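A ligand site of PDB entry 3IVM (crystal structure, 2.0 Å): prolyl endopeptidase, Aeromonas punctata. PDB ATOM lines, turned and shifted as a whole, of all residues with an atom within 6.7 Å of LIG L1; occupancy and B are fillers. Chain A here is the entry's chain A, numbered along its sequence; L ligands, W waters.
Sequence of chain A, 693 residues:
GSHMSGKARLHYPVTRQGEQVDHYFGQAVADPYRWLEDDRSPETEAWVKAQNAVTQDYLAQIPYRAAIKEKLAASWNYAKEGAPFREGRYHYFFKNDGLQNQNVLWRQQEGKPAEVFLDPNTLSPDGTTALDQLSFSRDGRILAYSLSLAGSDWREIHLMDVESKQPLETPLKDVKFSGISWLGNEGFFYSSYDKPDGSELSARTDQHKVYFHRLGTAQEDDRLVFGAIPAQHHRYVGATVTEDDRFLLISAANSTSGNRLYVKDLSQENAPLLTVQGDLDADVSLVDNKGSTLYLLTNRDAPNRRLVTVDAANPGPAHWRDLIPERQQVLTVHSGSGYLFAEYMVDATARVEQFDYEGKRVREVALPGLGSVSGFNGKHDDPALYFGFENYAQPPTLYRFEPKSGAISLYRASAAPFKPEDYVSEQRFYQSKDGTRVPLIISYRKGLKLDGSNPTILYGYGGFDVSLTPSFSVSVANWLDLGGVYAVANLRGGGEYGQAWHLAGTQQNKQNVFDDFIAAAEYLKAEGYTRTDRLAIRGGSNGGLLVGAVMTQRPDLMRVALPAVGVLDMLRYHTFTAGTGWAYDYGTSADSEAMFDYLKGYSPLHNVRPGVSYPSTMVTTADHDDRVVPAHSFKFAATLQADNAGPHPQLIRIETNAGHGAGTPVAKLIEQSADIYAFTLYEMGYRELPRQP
Thr 256 touches LIG L1.
CZ of Phe 464 touches C10 of LIG L1, 3.4 Å away.
Val 567 touches LIG L1 (CG2 to C7, 3.5 Å).
OH of Tyr 586 touches C8 of LIG L1, 3.4 Å away.
Val 628 touches LIG L1.
Hydrophobic or aromatic side chains that line LIG L1: Tyr 461, Phe 464, Val 567, Trp 582 and Val 628.
Ten residues have an atom within 4 Å of LIG L1: Thr 256, Tyr 461, Phe 464, Ser 541, Asn 542, Val 567, Trp 582, Tyr 586, Arg 627 and Val 628.
The nearest printed residue that does not touch LIG L1 is His 660 (4.02 Å).
NE2 of His 660 sits at hydrogen-bond distance from OG of Ser 541 (3.3 Å).
ND2 of Asn 542 sits at hydrogen-bond distance from OH of Tyr 586, at 2.6 Å.
NE of Arg 627 lies within salt-bridge range of OD1 of Asp 153, 2.8 Å away.
The backbone NH of Thr 256 lies within hydrogen-bond range of the backbone carbonyl oxygen of Gly 581.
The side-chain amide oxygen (OD1) of Asn 542 sits close to the backbone carbonyl oxygen (O) of Tyr 461 (3.1 Å).
O of Ser 541 lies within hydrogen-bond range of N of Val 567.
Water W3 lies within hydrogen-bond range of O2 of LIG L1 (2.7 Å), OH of Tyr 236 (2.7 Å), O of Ala 578 (3.4 Å) and NE1 of Trp 582 (3.5 Å).
Water W2 lies within hydrogen-bond range of a ring nitrogen (NE2) of His 660 (2.5 Å), an oxygen (O3) of LIG L1 (2.7 Å) and the side-chain hydroxyl of Ser 541 (3.2 Å).
Water W1 lies within hydrogen-bond range of the side-chain hydroxyl (OH) of Tyr 461 (2.6 Å) and an oxygen (O4) of LIG L1 (3.1 Å).
O4 of LIG L1 is in hydrogen-bond range of N of Asn 542.
The side-chain hydroxyl of Ser 541 is bonded to a carbon (C9) of LIG L1.
OH of Tyr 461 is in hydrogen-bond range of O4 of LIG L1.
The indole nitrogen of Trp 582 sits at hydrogen-bond distance from an oxygen (O2) of LIG L1, at 2.9 Å.
The guanidinium group (NH1) of Arg 627 lies within salt-bridge range of an oxygen (O1) of LIG L1 (3.7 Å).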
ATOM      1  N   ASP A 153      -9.960 -23.530 -12.296  1.00  0.00           N
ATOM      2  CA  ASP A 153      -9.575 -23.336 -13.683  1.00  0.00           C
ATOM      3  C   ASP A 153      -8.075 -23.668 -13.881  1.00  0.00           C
ATOM      4  O   ASP A 153      -7.595 -23.752 -15.010  1.00  0.00           O
ATOM      5  CB  ASP A 153      -9.846 -21.883 -14.123  1.00  0.00           C
ATOM      6  CG  ASP A 153     -11.283 -21.670 -14.614  1.00  0.00           C
ATOM      7  OD1 ASP A 153     -11.703 -20.497 -14.680  1.00  0.00           O
ATOM      8  OD2 ASP A 153     -11.974 -22.665 -14.939  1.00  0.00           O
ATOM      9  N   PHE A 177      -6.580 -22.465 -19.002  1.00  0.00           N
ATOM     10  CA  PHE A 177      -7.248 -22.101 -20.263  1.00  0.00           C
ATOM     11  C   PHE A 177      -6.301 -22.555 -21.363  1.00  0.00           C
ATOM     12  O   PHE A 177      -5.867 -21.768 -22.207  1.00  0.00           O
ATOM     13  CB  PHE A 177      -7.461 -20.577 -20.385  1.00  0.00           C
ATOM     14  CG  PHE A 177      -8.262 -19.964 -19.273  1.00  0.00           C
ATOM     15  CD1 PHE A 177      -9.388 -20.603 -18.754  1.00  0.00           C
ATOM     16  CD2 PHE A 177      -7.903 -18.720 -18.752  1.00  0.00           C
ATOM     17  CE1 PHE A 177     -10.135 -20.024 -17.733  1.00  0.00           C
ATOM     18  CE2 PHE A 177      -8.654 -18.129 -17.726  1.00  0.00           C
ATOM     19  CZ  PHE A 177      -9.767 -18.778 -17.210  1.00  0.00           C
ATOM     20  N   TYR A 236      -5.452 -14.012 -23.262  1.00  0.00           N
ATOM     21  CA  TYR A 236      -5.751 -15.386 -23.668  1.00  0.00           C
ATOM     22  C   TYR A 236      -5.026 -15.802 -24.943  1.00  0.00           C
ATOM     23  O   TYR A 236      -5.280 -15.234 -25.992  1.00  0.00           O
ATOM     24  CB  TYR A 236      -7.251 -15.589 -23.936  1.00  0.00           C
ATOM     25  CG  TYR A 236      -8.200 -15.144 -22.857  1.00  0.00           C
ATOM     26  CD1 TYR A 236      -8.264 -15.804 -21.638  1.00  0.00           C
ATOM     27  CD2 TYR A 236      -9.077 -14.073 -23.072  1.00  0.00           C
ATOM     28  CE1 TYR A 236      -9.173 -15.426 -20.646  1.00  0.00           C
ATOM     29  CE2 TYR A 236      -9.989 -13.676 -22.087  1.00  0.00           C
ATOM     30  CZ  TYR A 236     -10.022 -14.359 -20.883  1.00  0.00           C
ATOM     31  OH  TYR A 236     -10.917 -13.974 -19.910  1.00  0.00           O
ATOM     32  N   THR A 256     -13.314 -12.223 -24.421  1.00  0.00           N
ATOM     33  CA  THR A 256     -13.932 -13.467 -24.844  1.00  0.00           C
ATOM     34  C   THR A 256     -14.452 -13.406 -26.272  1.00  0.00           C
ATOM     35  O   THR A 256     -14.884 -14.418 -26.832  1.00  0.00           O
ATOM     36  CB  THR A 256     -15.063 -13.858 -23.874  1.00  0.00           C
ATOM     37  OG1 THR A 256     -16.032 -12.800 -23.809  1.00  0.00           O
ATOM     38  CG2 THR A 256     -14.478 -14.125 -22.483  1.00  0.00           C
ATOM     39  N   TYR A 461     -29.519 -17.077 -19.988  1.00  0.00           N
ATOM     40  CA  TYR A 461     -28.091 -16.737 -19.874  1.00  0.00           C
ATOM     41  C   TYR A 461     -28.004 -15.314 -20.424  1.00  0.00           C
ATOM     42  O   TYR A 461     -28.022 -14.366 -19.669  1.00  0.00           O
ATOM     43  CB  TYR A 461     -27.241 -17.694 -20.736  1.00  0.00           C
ATOM     44  CG  TYR A 461     -25.748 -17.551 -20.540  1.00  0.00           C
ATOM     45  CD1 TYR A 461     -25.108 -18.050 -19.402  1.00  0.00           C
ATOM     46  CD2 TYR A 461     -24.954 -16.941 -21.516  1.00  0.00           C
ATOM     47  CE1 TYR A 461     -23.716 -17.938 -19.243  1.00  0.00           C
ATOM     48  CE2 TYR A 461     -23.591 -16.827 -21.367  1.00  0.00           C
ATOM     49  CZ  TYR A 461     -22.971 -17.323 -20.237  1.00  0.00           C
ATOM     50  OH  TYR A 461     -21.595 -17.213 -20.137  1.00  0.00           O
ATOM     51  N   GLY A 463     -25.652 -13.538 -23.212  1.00  0.00           N
ATOM     52  CA  GLY A 463     -24.394 -12.846 -23.350  1.00  0.00           C
ATOM     53  C   GLY A 463     -23.273 -13.723 -23.856  1.00  0.00           C
ATOM     54  O   GLY A 463     -23.389 -14.947 -23.936  1.00  0.00           O
ATOM     55  N   PHE A 464     -22.181 -13.058 -24.229  1.00  0.00           N
ATOM     56  CA  PHE A 464     -20.975 -13.724 -24.671  1.00  0.00           C
ATOM     57  C   PHE A 464     -21.068 -14.612 -25.921  1.00  0.00           C
ATOM     58  O   PHE A 464     -20.239 -15.504 -26.116  1.00  0.00           O
ATOM     59  CB  PHE A 464     -20.438 -14.498 -23.464  1.00  0.00           C
ATOM     60  CG  PHE A 464     -20.038 -13.607 -22.329  1.00  0.00           C
ATOM     61  CD1 PHE A 464     -18.761 -13.032 -22.293  1.00  0.00           C
ATOM     62  CD2 PHE A 464     -20.951 -13.243 -21.345  1.00  0.00           C
ATOM     63  CE1 PHE A 464     -18.419 -12.106 -21.298  1.00  0.00           C
ATOM     64  CE2 PHE A 464     -20.618 -12.320 -20.353  1.00  0.00           C
ATOM     65  CZ  PHE A 464     -19.347 -11.750 -20.328  1.00  0.00           C
ATOM     66  N   VAL A 466     -23.072 -16.757 -26.484  1.00  0.00           N
ATOM     67  CA  VAL A 466     -23.388 -18.107 -26.035  1.00  0.00           C
ATOM     68  C   VAL A 466     -24.794 -18.477 -26.485  1.00  0.00           C
ATOM     69  O   VAL A 466     -25.725 -17.708 -26.342  1.00  0.00           O
ATOM     70  CB  VAL A 466     -23.323 -18.226 -24.483  1.00  0.00           C
ATOM     71  CG1 VAL A 466     -24.068 -19.472 -24.015  1.00  0.00           C
ATOM     72  CG2 VAL A 466     -21.874 -18.305 -24.016  1.00  0.00           C
ATOM     73  N   GLY A 540     -26.991 -19.015 -14.475  1.00  0.00           N
ATOM     74  CA  GLY A 540     -25.635 -19.243 -13.985  1.00  0.00           C
ATOM     75  C   GLY A 540     -24.542 -18.396 -14.632  1.00  0.00           C
ATOM     76  O   GLY A 540     -24.520 -18.241 -15.857  1.00  0.00           O
ATOM     77  N   SER A 541     -23.623 -17.892 -13.807  1.00  0.00           N
ATOM     78  CA  SER A 541     -22.524 -17.019 -14.262  1.00  0.00           C
ATOM     79  C   SER A 541     -23.064 -15.778 -14.797  1.00  0.00           C
ATOM     80  O   SER A 541     -23.603 -14.981 -14.023  1.00  0.00           O
ATOM     81  CB  SER A 541     -21.648 -17.762 -15.322  1.00  0.00           C
ATOM     82  OG  SER A 541     -20.332 -17.176 -15.484  1.00  0.00           O
ATOM     83  N   ASN A 542     -23.041 -15.622 -16.110  1.00  0.00           N
ATOM     84  CA  ASN A 542     -23.684 -14.478 -16.684  1.00  0.00           C
ATOM     85  C   ASN A 542     -25.177 -14.631 -16.459  1.00  0.00           C
ATOM     86  O   ASN A 542     -25.915 -13.640 -16.306  1.00  0.00           O
ATOM     87  CB  ASN A 542     -23.374 -14.352 -18.165  1.00  0.00           C
ATOM     88  CG  ASN A 542     -24.213 -13.299 -18.834  1.00  0.00           C
ATOM     89  OD1 ASN A 542     -25.062 -13.621 -19.666  1.00  0.00           O
ATOM     90  ND2 ASN A 542     -24.013 -12.040 -18.460  1.00  0.00           N
ATOM     91  N   GLY A 543     -25.635 -15.877 -16.431  1.00  0.00           N
ATOM     92  CA  GLY A 543     -27.052 -16.095 -16.182  1.00  0.00           C
ATOM     93  C   GLY A 543     -27.353 -15.779 -14.710  1.00  0.00           C
ATOM     94  O   GLY A 543     -28.509 -15.632 -14.327  1.00  0.00           O
ATOM     95  N   VAL A 565     -23.382 -19.117  -9.249  1.00  0.00           N
ATOM     96  CA  VAL A 565     -22.033 -18.594  -9.513  1.00  0.00           C
ATOM     97  C   VAL A 565     -22.072 -17.304 -10.341  1.00  0.00           C
ATOM     98  O   VAL A 565     -21.272 -17.117 -11.265  1.00  0.00           O
ATOM     99  CB  VAL A 565     -21.174 -19.649 -10.265  1.00  0.00           C
ATOM    100  CG1 VAL A 565     -20.812 -20.811  -9.332  1.00  0.00           C
ATOM    101  CG2 VAL A 565     -21.923 -20.166 -11.478  1.00  0.00           C
ATOM    102  N   GLY A 566     -22.978 -16.401  -9.988  1.00  0.00           N
ATOM    103  CA  GLY A 566     -23.154 -15.167 -10.725  1.00  0.00           C
ATOM    104  C   GLY A 566     -22.215 -13.995 -10.511  1.00  0.00           C
ATOM    105  O   GLY A 566     -21.595 -13.871  -9.456  1.00  0.00           O
ATOM    106  N   VAL A 567     -22.117 -13.146 -11.523  1.00  0.00           N
ATOM    107  CA  VAL A 567     -21.285 -11.942 -11.465  1.00  0.00           C
ATOM    108  C   VAL A 567     -22.266 -10.920 -10.866  1.00  0.00           C
ATOM    109  O   VAL A 567     -23.138 -10.423 -11.566  1.00  0.00           O
ATOM    110  CB  VAL A 567     -20.870 -11.482 -12.877  1.00  0.00           C
ATOM    111  CG1 VAL A 567     -19.788 -10.430 -12.798  1.00  0.00           C
ATOM    112  CG2 VAL A 567     -20.409 -12.671 -13.682  1.00  0.00           C
ATOM    113  N   ALA A 578      -9.647 -13.426 -14.143  1.00  0.00           N
ATOM    114  CA  ALA A 578      -9.620 -12.974 -15.533  1.00  0.00           C
ATOM    115  C   ALA A 578     -10.970 -12.361 -15.916  1.00  0.00           C
ATOM    116  O   ALA A 578     -11.463 -12.539 -17.032  1.00  0.00           O
ATOM    117  CB  ALA A 578      -9.270 -14.127 -16.485  1.00  0.00           C
ATOM    118  N   GLY A 581     -11.400 -10.086 -18.810  1.00  0.00           N
ATOM    119  CA  GLY A 581     -11.616 -10.735 -20.086  1.00  0.00           C
ATOM    120  C   GLY A 581     -13.061 -10.614 -20.530  1.00  0.00           C
ATOM    121  O   GLY A 581     -13.385 -11.012 -21.654  1.00  0.00           O
ATOM    122  N   TRP A 582     -13.936 -10.058 -19.689  1.00  0.00           N
ATOM    123  CA  TRP A 582     -15.351  -9.917 -20.064  1.00  0.00           C
ATOM    124  C   TRP A 582     -15.741  -8.478 -20.364  1.00  0.00           C
ATOM    125  O   TRP A 582     -16.920  -8.181 -20.539  1.00  0.00           O
ATOM    126  CB  TRP A 582     -16.278 -10.456 -18.946  1.00  0.00           C
ATOM    127  CG  TRP A 582     -15.866 -11.779 -18.365  1.00  0.00           C
ATOM    128  CD1 TRP A 582     -15.315 -12.838 -19.035  1.00  0.00           C
ATOM    129  CD2 TRP A 582     -15.940 -12.175 -16.976  1.00  0.00           C
ATOM    130  NE1 TRP A 582     -15.024 -13.857 -18.147  1.00  0.00           N
ATOM    131  CE2 TRP A 582     -15.396 -13.469 -16.886  1.00  0.00           C
ATOM    132  CE3 TRP A 582     -16.403 -11.550 -15.817  1.00  0.00           C
ATOM    133  CZ2 TRP A 582     -15.302 -14.156 -15.670  1.00  0.00           C
ATOM    134  CZ3 TRP A 582     -16.308 -12.231 -14.613  1.00  0.00           C
ATOM    135  CH2 TRP A 582     -15.760 -13.520 -14.545  1.00  0.00           C
ATOM    136  N   TYR A 586     -19.383  -6.542 -20.843  1.00  0.00           N
ATOM    137  CA  TYR A 586     -19.924  -5.704 -19.774  1.00  0.00           C
ATOM    138  C   TYR A 586     -19.433  -4.274 -19.670  1.00  0.00           C
ATOM    139  O   TYR A 586     -20.155  -3.403 -19.167  1.00  0.00           O
ATOM    140  CB  TYR A 586     -19.680  -6.350 -18.398  1.00  0.00           C
ATOM    141  CG  TYR A 586     -20.226  -7.744 -18.169  1.00  0.00           C
ATOM    142  CD1 TYR A 586     -21.473  -8.135 -18.634  1.00  0.00           C
ATOM    143  CD2 TYR A 586     -19.510  -8.650 -17.388  1.00  0.00           C
ATOM    144  CE1 TYR A 586     -21.998  -9.394 -18.339  1.00  0.00           C
ATOM    145  CE2 TYR A 586     -20.022  -9.899 -17.070  1.00  0.00           C
ATOM    146  CZ  TYR A 586     -21.263 -10.268 -17.539  1.00  0.00           C
ATOM    147  OH  TYR A 586     -21.764 -11.497 -17.202  1.00  0.00           O
ATOM    148  N   ARG A 627     -13.381 -18.638 -11.681  1.00  0.00           N
ATOM    149  CA  ARG A 627     -13.863 -18.064 -12.930  1.00  0.00           C
ATOM    150  C   ARG A 627     -14.554 -16.814 -12.410  1.00  0.00           C
ATOM    151  O   ARG A 627     -14.183 -15.695 -12.748  1.00  0.00           O
ATOM    152  CB  ARG A 627     -14.862 -18.988 -13.623  1.00  0.00           C
ATOM    153  CG  ARG A 627     -15.391 -18.466 -14.962  1.00  0.00           C
ATOM    154  CD  ARG A 627     -14.282 -18.301 -15.981  1.00  0.00           C
ATOM    155  NE  ARG A 627     -13.745 -19.595 -16.399  1.00  0.00           N
ATOM    156  CZ  ARG A 627     -14.257 -20.365 -17.355  1.00  0.00           C
ATOM    157  NH1 ARG A 627     -15.340 -19.982 -18.029  1.00  0.00           N
ATOM    158  NH2 ARG A 627     -13.718 -21.546 -17.609  1.00  0.00           N
ATOM    159  N   VAL A 628     -15.554 -17.037 -11.544  1.00  0.00           N
ATOM    160  CA  VAL A 628     -16.326 -15.978 -10.884  1.00  0.00           C
ATOM    161  C   VAL A 628     -16.109 -16.106  -9.375  1.00  0.00           C
ATOM    162  O   VAL A 628     -16.806 -16.869  -8.695  1.00  0.00           O
ATOM    163  CB  VAL A 628     -17.854 -16.135 -11.131  1.00  0.00           C
ATOM    164  CG1 VAL A 628     -18.634 -15.220 -10.211  1.00  0.00           C
ATOM    165  CG2 VAL A 628     -18.187 -15.826 -12.591  1.00  0.00           C
ATOM    166  N   HIS A 660     -16.347 -23.520 -10.537  1.00  0.00           N
ATOM    167  CA  HIS A 660     -17.385 -22.923 -11.358  1.00  0.00           C
ATOM    168  C   HIS A 660     -18.428 -23.905 -11.862  1.00  0.00           C
ATOM    169  O   HIS A 660     -19.594 -23.549 -12.029  1.00  0.00           O
ATOM    170  CB  HIS A 660     -16.769 -22.197 -12.550  1.00  0.00           C
ATOM    171  CG  HIS A 660     -17.718 -21.242 -13.228  1.00  0.00           C
ATOM    172  ND1 HIS A 660     -18.220 -20.132 -12.589  1.00  0.00           N
ATOM    173  CD2 HIS A 660     -18.229 -21.232 -14.472  1.00  0.00           C
ATOM    174  CE1 HIS A 660     -19.005 -19.465 -13.432  1.00  0.00           C
ATOM    175  NE2 HIS A 660     -19.030 -20.118 -14.575  1.00  0.00           N
HETATM  176  O1  LIG L   1     -13.620 -17.976 -20.642  1.00  0.00           O
HETATM  177  C1  LIG L   1     -14.601 -17.216 -20.140  1.00  0.00           C
HETATM  178  O2  LIG L   1     -14.388 -16.495 -19.173  1.00  0.00           O
HETATM  179  N1  LIG L   1     -15.847 -17.242 -20.703  1.00  0.00           N
HETATM  180  C2  LIG L   1     -17.051 -16.452 -20.276  1.00  0.00           C
HETATM  181  C3  LIG L   1     -17.494 -16.775 -18.860  1.00  0.00           C
HETATM  182  O3  LIG L   1     -17.225 -17.861 -18.388  1.00  0.00           O
HETATM  183  C4  LIG L   1     -18.190 -16.832 -21.246  1.00  0.00           C
HETATM  184  C5  LIG L   1     -17.777 -18.231 -21.774  1.00  0.00           C
HETATM  185  C6  LIG L   1     -16.236 -18.058 -21.878  1.00  0.00           C
HETATM  186  C7  LIG L   1     -18.855 -14.670 -16.143  1.00  0.00           C
HETATM  187  C8  LIG L   1     -19.345 -13.853 -17.369  1.00  0.00           C
HETATM  188  C9  LIG L   1     -20.029 -16.837 -16.668  1.00  0.00           C
HETATM  189  O4  LIG L   1     -20.686 -17.035 -17.670  1.00  0.00           O
HETATM  190  N2  LIG L   1     -18.185 -15.871 -18.103  1.00  0.00           N
HETATM  191  C10 LIG L   1     -18.581 -14.514 -18.536  1.00  0.00           C
HETATM  192  C11 LIG L   1     -18.682 -16.085 -16.716  1.00  0.00           C
HETATM  193  C1  LG2 L   2     -24.093 -21.716 -16.111  1.00  0.00           C
HETATM  194  C2  LG2 L   2     -22.788 -21.407 -16.557  1.00  0.00           C
HETATM  195  C3  LG2 L   2     -21.675 -21.663 -15.725  1.00  0.00           C
HETATM  196  C4  LG2 L   2     -21.852 -22.237 -14.449  1.00  0.00           C
HETATM  197  C5  LG2 L   2     -23.160 -22.544 -13.994  1.00  0.00           C
HETATM  198  C6  LG2 L   2     -24.276 -22.285 -14.817  1.00  0.00           C
HETATM  199  C7  LG2 L   2     -25.661 -22.608 -14.339  1.00  0.00           C
HETATM  200  O1  LG2 L   2     -26.197 -23.751 -15.061  1.00  0.00           O
HETATM  201  C8  LG2 L   2     -27.455 -24.214 -14.794  1.00  0.00           C
HETATM  202  O2  LG2 L   2     -28.133 -23.641 -13.946  1.00  0.00           O
HETATM  203  N1  LG2 L   2     -27.962 -25.305 -15.477  1.00  0.00           N
HETATM  204  C9  LG2 L   2     -29.307 -25.921 -15.294  1.00  0.00           C
HETATM  205  C10 LG2 L   2     -29.520 -26.306 -13.834  1.00  0.00           C
HETATM  206  O3  LG2 L   2     -28.556 -26.603 -13.162  1.00  0.00           O
HETATM  207  C11 LG2 L   2     -29.412 -27.117 -16.258  1.00  0.00           C
HETATM  208  C12 LG2 L   2     -27.921 -27.473 -16.518  1.00  0.00           C
HETATM  209  C13 LG2 L   2     -27.245 -26.070 -16.519  1.00  0.00           C
HETATM  210  C14 LG2 L   2     -32.540 -26.206 -11.550  1.00  0.00           C
HETATM  211  C15 LG2 L   2     -33.205 -26.107 -12.951  1.00  0.00           C
HETATM  212  C16 LG2 L   2     -30.840 -28.105 -11.530  1.00  0.00           C
HETATM  213  O4  LG2 L   2     -29.994 -28.398 -10.701  1.00  0.00           O
HETATM  214  N2  LG2 L   2     -30.780 -26.305 -13.267  1.00  0.00           N
HETATM  215  C17 LG2 L   2     -32.039 -25.969 -13.954  1.00  0.00           C
HETATM  216  C18 LG2 L   2     -31.074 -26.641 -11.839  1.00  0.00           C
HETATM  217  O   HOH W   1     -20.600 -19.540 -19.550  1.00  0.00           O
HETATM  218  O   HOH W   2     -18.814 -19.589 -17.010  1.00  0.00           O
HETATM  219  O   HOH W   3     -12.058 -15.681 -18.099  1.00  0.00           O
